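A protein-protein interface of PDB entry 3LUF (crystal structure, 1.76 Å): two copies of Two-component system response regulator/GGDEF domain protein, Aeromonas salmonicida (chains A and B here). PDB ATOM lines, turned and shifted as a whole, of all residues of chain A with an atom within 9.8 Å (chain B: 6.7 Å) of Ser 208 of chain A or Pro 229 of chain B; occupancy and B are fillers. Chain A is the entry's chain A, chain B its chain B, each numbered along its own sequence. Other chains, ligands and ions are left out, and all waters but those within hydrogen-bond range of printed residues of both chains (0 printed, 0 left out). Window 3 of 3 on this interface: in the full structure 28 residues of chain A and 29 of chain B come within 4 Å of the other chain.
OG of Ser 208 of chain A is in hydrogen-bond range of OE2 of Glu 234 of chain B.
The side-chain hydroxyl (OG) of Ser 208 of chain A sits at hydrogen-bond distance from the backbone carbonyl oxygen (O) of Pro 229 of chain B.
The side-chain carboxylate of Glu 234 of chain B is in hydrogen-bond range of the side-chain hydroxyl of Ser 214 of chain A, at 2.8 Å.
The side-chain amide nitrogen of Asn 227 of chain A lies within hydrogen-bond range of the side-chain carboxylate of Glu 234 of chain B.
OG of Ser 206 of chain A is in hydrogen-bond range of OD1 of Asn 227 of chain A (3.2 Å).
N of Glu 231 of chain B is in hydrogen-bond range of OE2 of Glu 234 of chain B.
The backbone NH of Val 207 of chain A lies close to the side-chain amide oxygen of Asn 227 of chain A, at 3.5 Å.
OG of Ser 206 of chain A is in hydrogen-bond range of OG of Ser 214 of chain A, 2.9 Å away.
CA of Phe 230 of chain B touches OG of Ser 208 of chain A, 3.9 Å away.
Glu 234 of chain B touches Phe 225 of chain A.
Of chain B, only Pro 229 (3.2 Å), Phe 230 (3.9 Å) and Glu 234 (2.8 Å) come within 4 Å of Ser 208 of chain A.
Printed residues of chain B within 4 Å of Ser 214 of chain A: Glu 234.
Printed residues of chain B within 4 Å of Phe 225 of chain A: Glu 234 (3.5 Å).
Pro 229 of chain B touches just one residue of chain A: Ser 208 (3.2 Å).
Glu 231 of chain B touches none of the printed residues of chain A.
Of the printed residues of chain A, Glu 234 of chain B touches Ser 208 (2.8 Å), Ser 214 (2.8 Å), Phe 225 (3.5 Å) and Asn 227 (3.1 Å).
The nearest residue of chain B that does not touch Ser 208 of chain A is Glu 231 of chain B (4.4 Å).
The nearest printed residue of chain B that does not touch Asn 227 of chain A is Pro 229 of chain B (5.7 Å).
Among the printed residues, no Asp or Glu carboxylate lies within 4 Å of a Lys or Arg side-chain nitrogen of the other chain.
6 positions are printed for both chains.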
ATOM      1  N   TYR A 177      28.725  -6.257 -26.761  1.00  0.00           N
ATOM      2  CA  TYR A 177      28.967  -6.213 -28.204  1.00  0.00           C
ATOM      3  C   TYR A 177      30.427  -6.144 -28.634  1.00  0.00           C
ATOM      4  O   TYR A 177      30.815  -6.842 -29.577  1.00  0.00           O
ATOM      5  CB  TYR A 177      28.139  -5.092 -28.855  1.00  0.00           C
ATOM      6  CG  TYR A 177      28.417  -3.703 -28.290  1.00  0.00           C
ATOM      7  CD1 TYR A 177      29.326  -2.869 -28.907  1.00  0.00           C
ATOM      8  CD2 TYR A 177      27.730  -3.220 -27.169  1.00  0.00           C
ATOM      9  CE1 TYR A 177      29.570  -1.587 -28.429  1.00  0.00           C
ATOM     10  CE2 TYR A 177      27.984  -1.919 -26.670  1.00  0.00           C
ATOM     11  CZ  TYR A 177      28.905  -1.121 -27.320  1.00  0.00           C
ATOM     12  OH  TYR A 177      29.184   0.172 -26.876  1.00  0.00           O
ATOM     13  N   GLY A 204      21.537 -10.070 -26.226  1.00  0.00           N
ATOM     14  CA  GLY A 204      22.608  -9.250 -26.753  1.00  0.00           C
ATOM     15  C   GLY A 204      22.548  -7.850 -26.199  1.00  0.00           C
ATOM     16  O   GLY A 204      21.536  -7.163 -26.306  1.00  0.00           O
ATOM     17  N   ILE A 205      23.661  -7.420 -25.602  1.00  0.00           N
ATOM     18  CA  ILE A 205      23.776  -6.055 -25.099  1.00  0.00           C
ATOM     19  C   ILE A 205      24.181  -5.173 -26.244  1.00  0.00           C
ATOM     20  O   ILE A 205      25.205  -5.395 -26.885  1.00  0.00           O
ATOM     21  CB  ILE A 205      24.767  -5.922 -23.915  1.00  0.00           C
ATOM     22  CG1 ILE A 205      24.347  -6.845 -22.754  1.00  0.00           C
ATOM     23  CG2 ILE A 205      24.842  -4.430 -23.490  1.00  0.00           C
ATOM     24  CD1 ILE A 205      22.900  -6.656 -22.249  1.00  0.00           C
ATOM     25  N   SER A 206      23.368  -4.161 -26.513  1.00  0.00           N
ATOM     26  CA  SER A 206      23.548  -3.371 -27.717  1.00  0.00           C
ATOM     27  C   SER A 206      23.499  -1.882 -27.423  1.00  0.00           C
ATOM     28  O   SER A 206      23.501  -1.470 -26.274  1.00  0.00           O
ATOM     29  CB  SER A 206      22.522  -3.773 -28.787  1.00  0.00           C
ATOM     30  OG  SER A 206      21.342  -4.277 -28.189  1.00  0.00           O
ATOM     31  N   VAL A 207      23.524  -1.090 -28.483  1.00  0.00           N
ATOM     32  CA  VAL A 207      23.338   0.336 -28.395  1.00  0.00           C
ATOM     33  C   VAL A 207      22.386   0.662 -29.527  1.00  0.00           C
ATOM     34  O   VAL A 207      22.438   0.041 -30.603  1.00  0.00           O
ATOM     35  CB  VAL A 207      24.655   1.168 -28.479  1.00  0.00           C
ATOM     36  CG1 VAL A 207      24.847   1.982 -27.201  1.00  0.00           C
ATOM     37  CG2 VAL A 207      25.880   0.306 -28.774  1.00  0.00           C
ATOM     38  N   SER A 208      21.469   1.580 -29.252  1.00  0.00           N
ATOM     39  CA  SER A 208      20.519   2.018 -30.261  1.00  0.00           C
ATOM     40  C   SER A 208      21.144   3.212 -30.990  1.00  0.00           C
ATOM     41  O   SER A 208      20.563   3.734 -31.935  1.00  0.00           O
ATOM     42  CB  SER A 208      19.151   2.348 -29.634  1.00  0.00           C
ATOM     43  OG  SER A 208      18.084   1.860 -30.441  1.00  0.00           O
ATOM     44  N   ASP A 209      22.332   3.637 -30.549  1.00  0.00           N
ATOM     45  CA  ASP A 209      23.166   4.551 -31.346  1.00  0.00           C
ATOM     46  C   ASP A 209      24.000   3.720 -32.324  1.00  0.00           C
ATOM     47  O   ASP A 209      25.211   3.601 -32.162  1.00  0.00           O
ATOM     48  CB  ASP A 209      24.081   5.404 -30.448  1.00  0.00           C
ATOM     49  N   LYS A 210      23.351   3.120 -33.323  1.00  0.00           N
ATOM     50  CA  LYS A 210      24.080   2.258 -34.268  1.00  0.00           C
ATOM     51  C   LYS A 210      23.380   1.752 -35.539  1.00  0.00           C
ATOM     52  O   LYS A 210      22.138   1.788 -35.679  1.00  0.00           O
ATOM     53  CB  LYS A 210      24.736   1.071 -33.558  1.00  0.00           C
ATOM     54  CG  LYS A 210      26.255   1.137 -33.589  1.00  0.00           C
ATOM     55  CD  LYS A 210      26.861   0.081 -32.729  1.00  0.00           C
ATOM     56  CE  LYS A 210      28.139   0.591 -32.110  1.00  0.00           C
ATOM     57  NZ  LYS A 210      27.817   1.670 -31.144  1.00  0.00           N
ATOM     58  N   ARG A 211      24.241   1.252 -36.436  1.00  0.00           N
ATOM     59  CA  ARG A 211      23.861   0.514 -37.625  1.00  0.00           C
ATOM     60  C   ARG A 211      23.364  -0.862 -37.205  1.00  0.00           C
ATOM     61  O   ARG A 211      24.027  -1.887 -37.435  1.00  0.00           O
ATOM     62  CB  ARG A 211      25.063   0.377 -38.575  1.00  0.00           C
ATOM     63  N   GLY A 212      22.213  -0.868 -36.540  1.00  0.00           N
ATOM     64  CA  GLY A 212      21.451  -2.075 -36.313  1.00  0.00           C
ATOM     65  C   GLY A 212      22.188  -3.237 -35.683  1.00  0.00           C
ATOM     66  O   GLY A 212      22.070  -4.383 -36.136  1.00  0.00           O
ATOM     67  N   LEU A 213      22.944  -2.945 -34.635  1.00  0.00           N
ATOM     68  CA  LEU A 213      23.551  -3.992 -33.825  1.00  0.00           C
ATOM     69  C   LEU A 213      22.510  -4.941 -33.216  1.00  0.00           C
ATOM     70  O   LEU A 213      22.735  -6.161 -33.130  1.00  0.00           O
ATOM     71  CB  LEU A 213      24.379  -3.328 -32.728  1.00  0.00           C
ATOM     72  CG  LEU A 213      25.323  -4.050 -31.807  1.00  0.00           C
ATOM     73  CD1 LEU A 213      26.342  -4.882 -32.601  1.00  0.00           C
ATOM     74  CD2 LEU A 213      26.016  -2.978 -30.968  1.00  0.00           C
ATOM     75  N   SER A 214      21.361  -4.403 -32.788  1.00  0.00           N
ATOM     76  CA  SER A 214      20.326  -5.278 -32.225  1.00  0.00           C
ATOM     77  C   SER A 214      19.816  -6.256 -33.268  1.00  0.00           C
ATOM     78  O   SER A 214      19.673  -7.446 -32.992  1.00  0.00           O
ATOM     79  CB  SER A 214      19.160  -4.488 -31.615  1.00  0.00           C
ATOM     80  OG  SER A 214      19.629  -3.815 -30.470  1.00  0.00           O
ATOM     81  N   ALA A 215      19.493  -5.741 -34.454  1.00  0.00           N
ATOM     82  CA  ALA A 215      19.103  -6.597 -35.581  1.00  0.00           C
ATOM     83  C   ALA A 215      20.114  -7.722 -35.839  1.00  0.00           C
ATOM     84  O   ALA A 215      19.725  -8.871 -36.016  1.00  0.00           O
ATOM     85  CB  ALA A 215      18.863  -5.740 -36.865  1.00  0.00           C
ATOM     86  N   TYR A 217      22.307  -9.108 -33.798  1.00  0.00           N
ATOM     87  CA  TYR A 217      22.183 -10.090 -32.712  1.00  0.00           C
ATOM     88  C   TYR A 217      21.023 -11.021 -32.952  1.00  0.00           C
ATOM     89  O   TYR A 217      21.156 -12.230 -32.822  1.00  0.00           O
ATOM     90  CB  TYR A 217      21.888  -9.404 -31.393  1.00  0.00           C
ATOM     91  CG  TYR A 217      23.092  -8.979 -30.580  1.00  0.00           C
ATOM     92  CD1 TYR A 217      24.046  -9.906 -30.178  1.00  0.00           C
ATOM     93  CD2 TYR A 217      23.212  -7.674 -30.178  1.00  0.00           C
ATOM     94  CE1 TYR A 217      25.135  -9.512 -29.378  1.00  0.00           C
ATOM     95  CE2 TYR A 217      24.280  -7.257 -29.388  1.00  0.00           C
ATOM     96  CZ  TYR A 217      25.234  -8.183 -29.013  1.00  0.00           C
ATOM     97  OH  TYR A 217      26.278  -7.786 -28.223  1.00  0.00           O
ATOM     98  N   PHE A 225      17.355  -8.421 -27.158  1.00  0.00           N
ATOM     99  CA  PHE A 225      18.372  -7.382 -27.040  1.00  0.00           C
ATOM    100  C   PHE A 225      18.085  -6.529 -25.797  1.00  0.00           C
ATOM    101  O   PHE A 225      16.950  -6.420 -25.339  1.00  0.00           O
ATOM    102  CB  PHE A 225      18.372  -6.485 -28.291  1.00  0.00           C
ATOM    103  CG  PHE A 225      17.151  -5.580 -28.367  1.00  0.00           C
ATOM    104  CD1 PHE A 225      15.954  -6.052 -28.886  1.00  0.00           C
ATOM    105  CD2 PHE A 225      17.203  -4.270 -27.892  1.00  0.00           C
ATOM    106  CE1 PHE A 225      14.806  -5.212 -28.919  1.00  0.00           C
ATOM    107  CE2 PHE A 225      16.078  -3.445 -27.915  1.00  0.00           C
ATOM    108  CZ  PHE A 225      14.877  -3.925 -28.438  1.00  0.00           C
ATOM    109  N   LEU A 226      19.109  -5.840 -25.318  1.00  0.00           N
ATOM    110  CA  LEU A 226      18.950  -4.865 -24.232  1.00  0.00           C
ATOM    111  C   LEU A 226      19.954  -3.764 -24.518  1.00  0.00           C
ATOM    112  O   LEU A 226      21.174  -4.016 -24.589  1.00  0.00           O
ATOM    113  CB  LEU A 226      19.214  -5.516 -22.866  1.00  0.00           C
ATOM    114  CG  LEU A 226      19.147  -4.542 -21.671  1.00  0.00           C
ATOM    115  CD1 LEU A 226      17.737  -4.038 -21.527  1.00  0.00           C
ATOM    116  CD2 LEU A 226      19.584  -5.268 -20.376  1.00  0.00           C
ATOM    117  N   ASN A 227      19.457  -2.545 -24.676  1.00  0.00           N
ATOM    118  CA  ASN A 227      20.307  -1.417 -25.007  1.00  0.00           C
ATOM    119  C   ASN A 227      20.969  -0.783 -23.786  1.00  0.00           C
ATOM    120  O   ASN A 227      20.332  -0.623 -22.759  1.00  0.00           O
ATOM    121  CB  ASN A 227      19.480  -0.389 -25.792  1.00  0.00           C
ATOM    122  CG  ASN A 227      19.214  -0.825 -27.227  1.00  0.00           C
ATOM    123  OD1 ASN A 227      20.096  -1.376 -27.892  1.00  0.00           O
ATOM    124  ND2 ASN A 227      18.020  -0.535 -27.730  1.00  0.00           N
ATOM    125  N   GLN A 228      22.258  -0.474 -23.904  1.00  0.00           N
ATOM    126  CA  GLN A 228      23.000   0.257 -22.876  1.00  0.00           C
ATOM    127  C   GLN A 228      22.945   1.744 -23.153  1.00  0.00           C
ATOM    128  O   GLN A 228      22.883   2.130 -24.304  1.00  0.00           O
ATOM    129  CB  GLN A 228      24.458  -0.211 -22.812  1.00  0.00           C
ATOM    130  CG  GLN A 228      24.634  -1.262 -21.731  1.00  0.00           C
ATOM    131  CD  GLN A 228      26.025  -1.828 -21.641  1.00  0.00           C
ATOM    132  OE1 GLN A 228      26.759  -1.870 -22.632  1.00  0.00           O
ATOM    133  NE2 GLN A 228      26.390  -2.302 -20.456  1.00  0.00           N
ATOM    134  N   PRO A 229      22.920   2.578 -22.095  1.00  0.00           N
ATOM    135  CA  PRO A 229      22.820   2.193 -20.687  1.00  0.00           C
ATOM    136  C   PRO A 229      21.401   1.732 -20.351  1.00  0.00           C
ATOM    137  O   PRO A 229      20.416   2.201 -20.944  1.00  0.00           O
ATOM    138  CB  PRO A 229      23.159   3.505 -19.942  1.00  0.00           C
ATOM    139  CG  PRO A 229      22.834   4.579 -20.895  1.00  0.00           C
ATOM    140  CD  PRO A 229      23.164   4.025 -22.248  1.00  0.00           C
ATOM    141  N   SER B 206       9.262   5.668 -24.375  1.00  0.00           N
ATOM    142  CA  SER B 206       9.831   6.785 -23.637  1.00  0.00           C
ATOM    143  C   SER B 206      11.159   7.208 -24.254  1.00  0.00           C
ATOM    144  O   SER B 206      11.855   6.383 -24.806  1.00  0.00           O
ATOM    145  CB  SER B 206      10.152   6.296 -22.215  1.00  0.00           C
ATOM    146  OG  SER B 206       9.405   7.043 -21.328  1.00  0.00           O
ATOM    147  N   VAL B 207      11.547   8.477 -24.107  1.00  0.00           N
ATOM    148  CA  VAL B 207      12.982   8.793 -24.215  1.00  0.00           C
ATOM    149  C   VAL B 207      13.602   8.491 -22.847  1.00  0.00           C
ATOM    150  O   VAL B 207      12.998   8.798 -21.802  1.00  0.00           O
ATOM    151  CB  VAL B 207      13.248  10.246 -24.659  1.00  0.00           C
ATOM    152  CG1 VAL B 207      12.792  10.445 -26.094  1.00  0.00           C
ATOM    153  CG2 VAL B 207      12.569  11.211 -23.735  1.00  0.00           C
ATOM    154  N   LEU B 226      10.116   0.364 -24.428  1.00  0.00           N
ATOM    155  CA  LEU B 226      10.897   0.523 -25.644  1.00  0.00           C
ATOM    156  C   LEU B 226      11.337   1.971 -25.666  1.00  0.00           C
ATOM    157  O   LEU B 226      10.505   2.888 -25.629  1.00  0.00           O
ATOM    158  CB  LEU B 226      10.040   0.155 -26.862  1.00  0.00           C
ATOM    159  CG  LEU B 226      10.635   0.393 -28.247  1.00  0.00           C
ATOM    160  CD1 LEU B 226      11.878  -0.428 -28.371  1.00  0.00           C
ATOM    161  CD2 LEU B 226       9.571   0.000 -29.293  1.00  0.00           C
ATOM    162  N   ASN B 227      12.649   2.193 -25.642  1.00  0.00           N
ATOM    163  CA  ASN B 227      13.154   3.549 -25.569  1.00  0.00           C
ATOM    164  C   ASN B 227      13.377   4.146 -26.960  1.00  0.00           C
ATOM    165  O   ASN B 227      13.840   3.460 -27.866  1.00  0.00           O
ATOM    166  CB  ASN B 227      14.411   3.621 -24.687  1.00  0.00           C
ATOM    167  CG  ASN B 227      14.120   3.257 -23.223  1.00  0.00           C
ATOM    168  OD1 ASN B 227      13.038   3.582 -22.674  1.00  0.00           O
ATOM    169  ND2 ASN B 227      15.078   2.585 -22.584  1.00  0.00           N
ATOM    170  N   GLN B 228      12.985   5.407 -27.136  1.00  0.00           N
ATOM    171  CA  GLN B 228      13.194   6.124 -28.406  1.00  0.00           C
ATOM    172  C   GLN B 228      14.532   6.863 -28.350  1.00  0.00           C
ATOM    173  O   GLN B 228      14.932   7.316 -27.282  1.00  0.00           O
ATOM    174  CB  GLN B 228      12.098   7.174 -28.610  1.00  0.00           C
ATOM    175  CG  GLN B 228      10.775   6.685 -29.164  1.00  0.00           C
ATOM    176  CD  GLN B 228       9.760   7.819 -29.310  1.00  0.00           C
ATOM    177  OE1 GLN B 228       9.936   8.903 -28.731  1.00  0.00           O
ATOM    178  NE2 GLN B 228       8.689   7.577 -30.091  1.00  0.00           N
ATOM    179  N   PRO B 229      15.252   6.972 -29.489  1.00  0.00           N
ATOM    180  CA  PRO B 229      15.020   6.333 -30.793  1.00  0.00           C
ATOM    181  C   PRO B 229      15.205   4.810 -30.788  1.00  0.00           C
ATOM    182  O   PRO B 229      16.049   4.305 -30.054  1.00  0.00           O
ATOM    183  CB  PRO B 229      16.105   6.960 -31.703  1.00  0.00           C
ATOM    184  CG  PRO B 229      17.189   7.427 -30.750  1.00  0.00           C
ATOM    185  CD  PRO B 229      16.391   7.914 -29.534  1.00  0.00           C
ATOM    186  N   PHE B 230      14.415   4.109 -31.601  1.00  0.00           N
ATOM    187  CA  PHE B 230      14.562   2.663 -31.828  1.00  0.00           C
ATOM    188  C   PHE B 230      14.508   2.330 -33.317  1.00  0.00           C
ATOM    189  O   PHE B 230      13.924   3.088 -34.126  1.00  0.00           O
ATOM    190  CB  PHE B 230      13.489   1.850 -31.062  1.00  0.00           C
ATOM    191  CG  PHE B 230      12.063   2.251 -31.400  1.00  0.00           C
ATOM    192  CD1 PHE B 230      11.426   1.731 -32.535  1.00  0.00           C
ATOM    193  CD2 PHE B 230      11.375   3.153 -30.595  1.00  0.00           C
ATOM    194  CE1 PHE B 230      10.123   2.106 -32.853  1.00  0.00           C
ATOM    195  CE2 PHE B 230      10.080   3.552 -30.913  1.00  0.00           C
ATOM    196  CZ  PHE B 230       9.458   3.030 -32.047  1.00  0.00           C
ATOM    197  N   GLU B 231      15.108   1.187 -33.669  1.00  0.00           N
ATOM    198  CA  GLU B 231      15.106   0.663 -35.027  1.00  0.00           C
ATOM    199  C   GLU B 231      13.900  -0.254 -35.253  1.00  0.00           C
ATOM    200  O   GLU B 231      13.373  -0.826 -34.280  1.00  0.00           O
ATOM    201  CB  GLU B 231      16.399  -0.112 -35.254  1.00  0.00           C
ATOM    202  CG  GLU B 231      17.657   0.759 -35.062  1.00  0.00           C
ATOM    203  CD  GLU B 231      17.823   1.816 -36.160  1.00  0.00           C
ATOM    204  OE1 GLU B 231      17.571   1.520 -37.354  1.00  0.00           O
ATOM    205  OE2 GLU B 231      18.198   2.954 -35.812  1.00  0.00           O
ATOM    206  N   GLU B 234      14.107  -3.643 -33.639  1.00  0.00           N
ATOM    207  CA  GLU B 234      13.905  -3.573 -32.203  1.00  0.00           C
ATOM    208  C   GLU B 234      12.409  -3.552 -31.881  1.00  0.00           C
ATOM    209  O   GLU B 234      11.942  -4.347 -31.060  1.00  0.00           O
ATOM    210  CB  GLU B 234      14.621  -2.377 -31.608  1.00  0.00           C
ATOM    211  CG  GLU B 234      16.138  -2.595 -31.582  1.00  0.00           C
ATOM    212  CD  GLU B 234      16.904  -1.354 -31.145  1.00  0.00           C
ATOM    213  OE1 GLU B 234      18.045  -1.516 -30.657  1.00  0.00           O
ATOM    214  OE2 GLU B 234      16.384  -0.229 -31.329  1.00  0.00           O
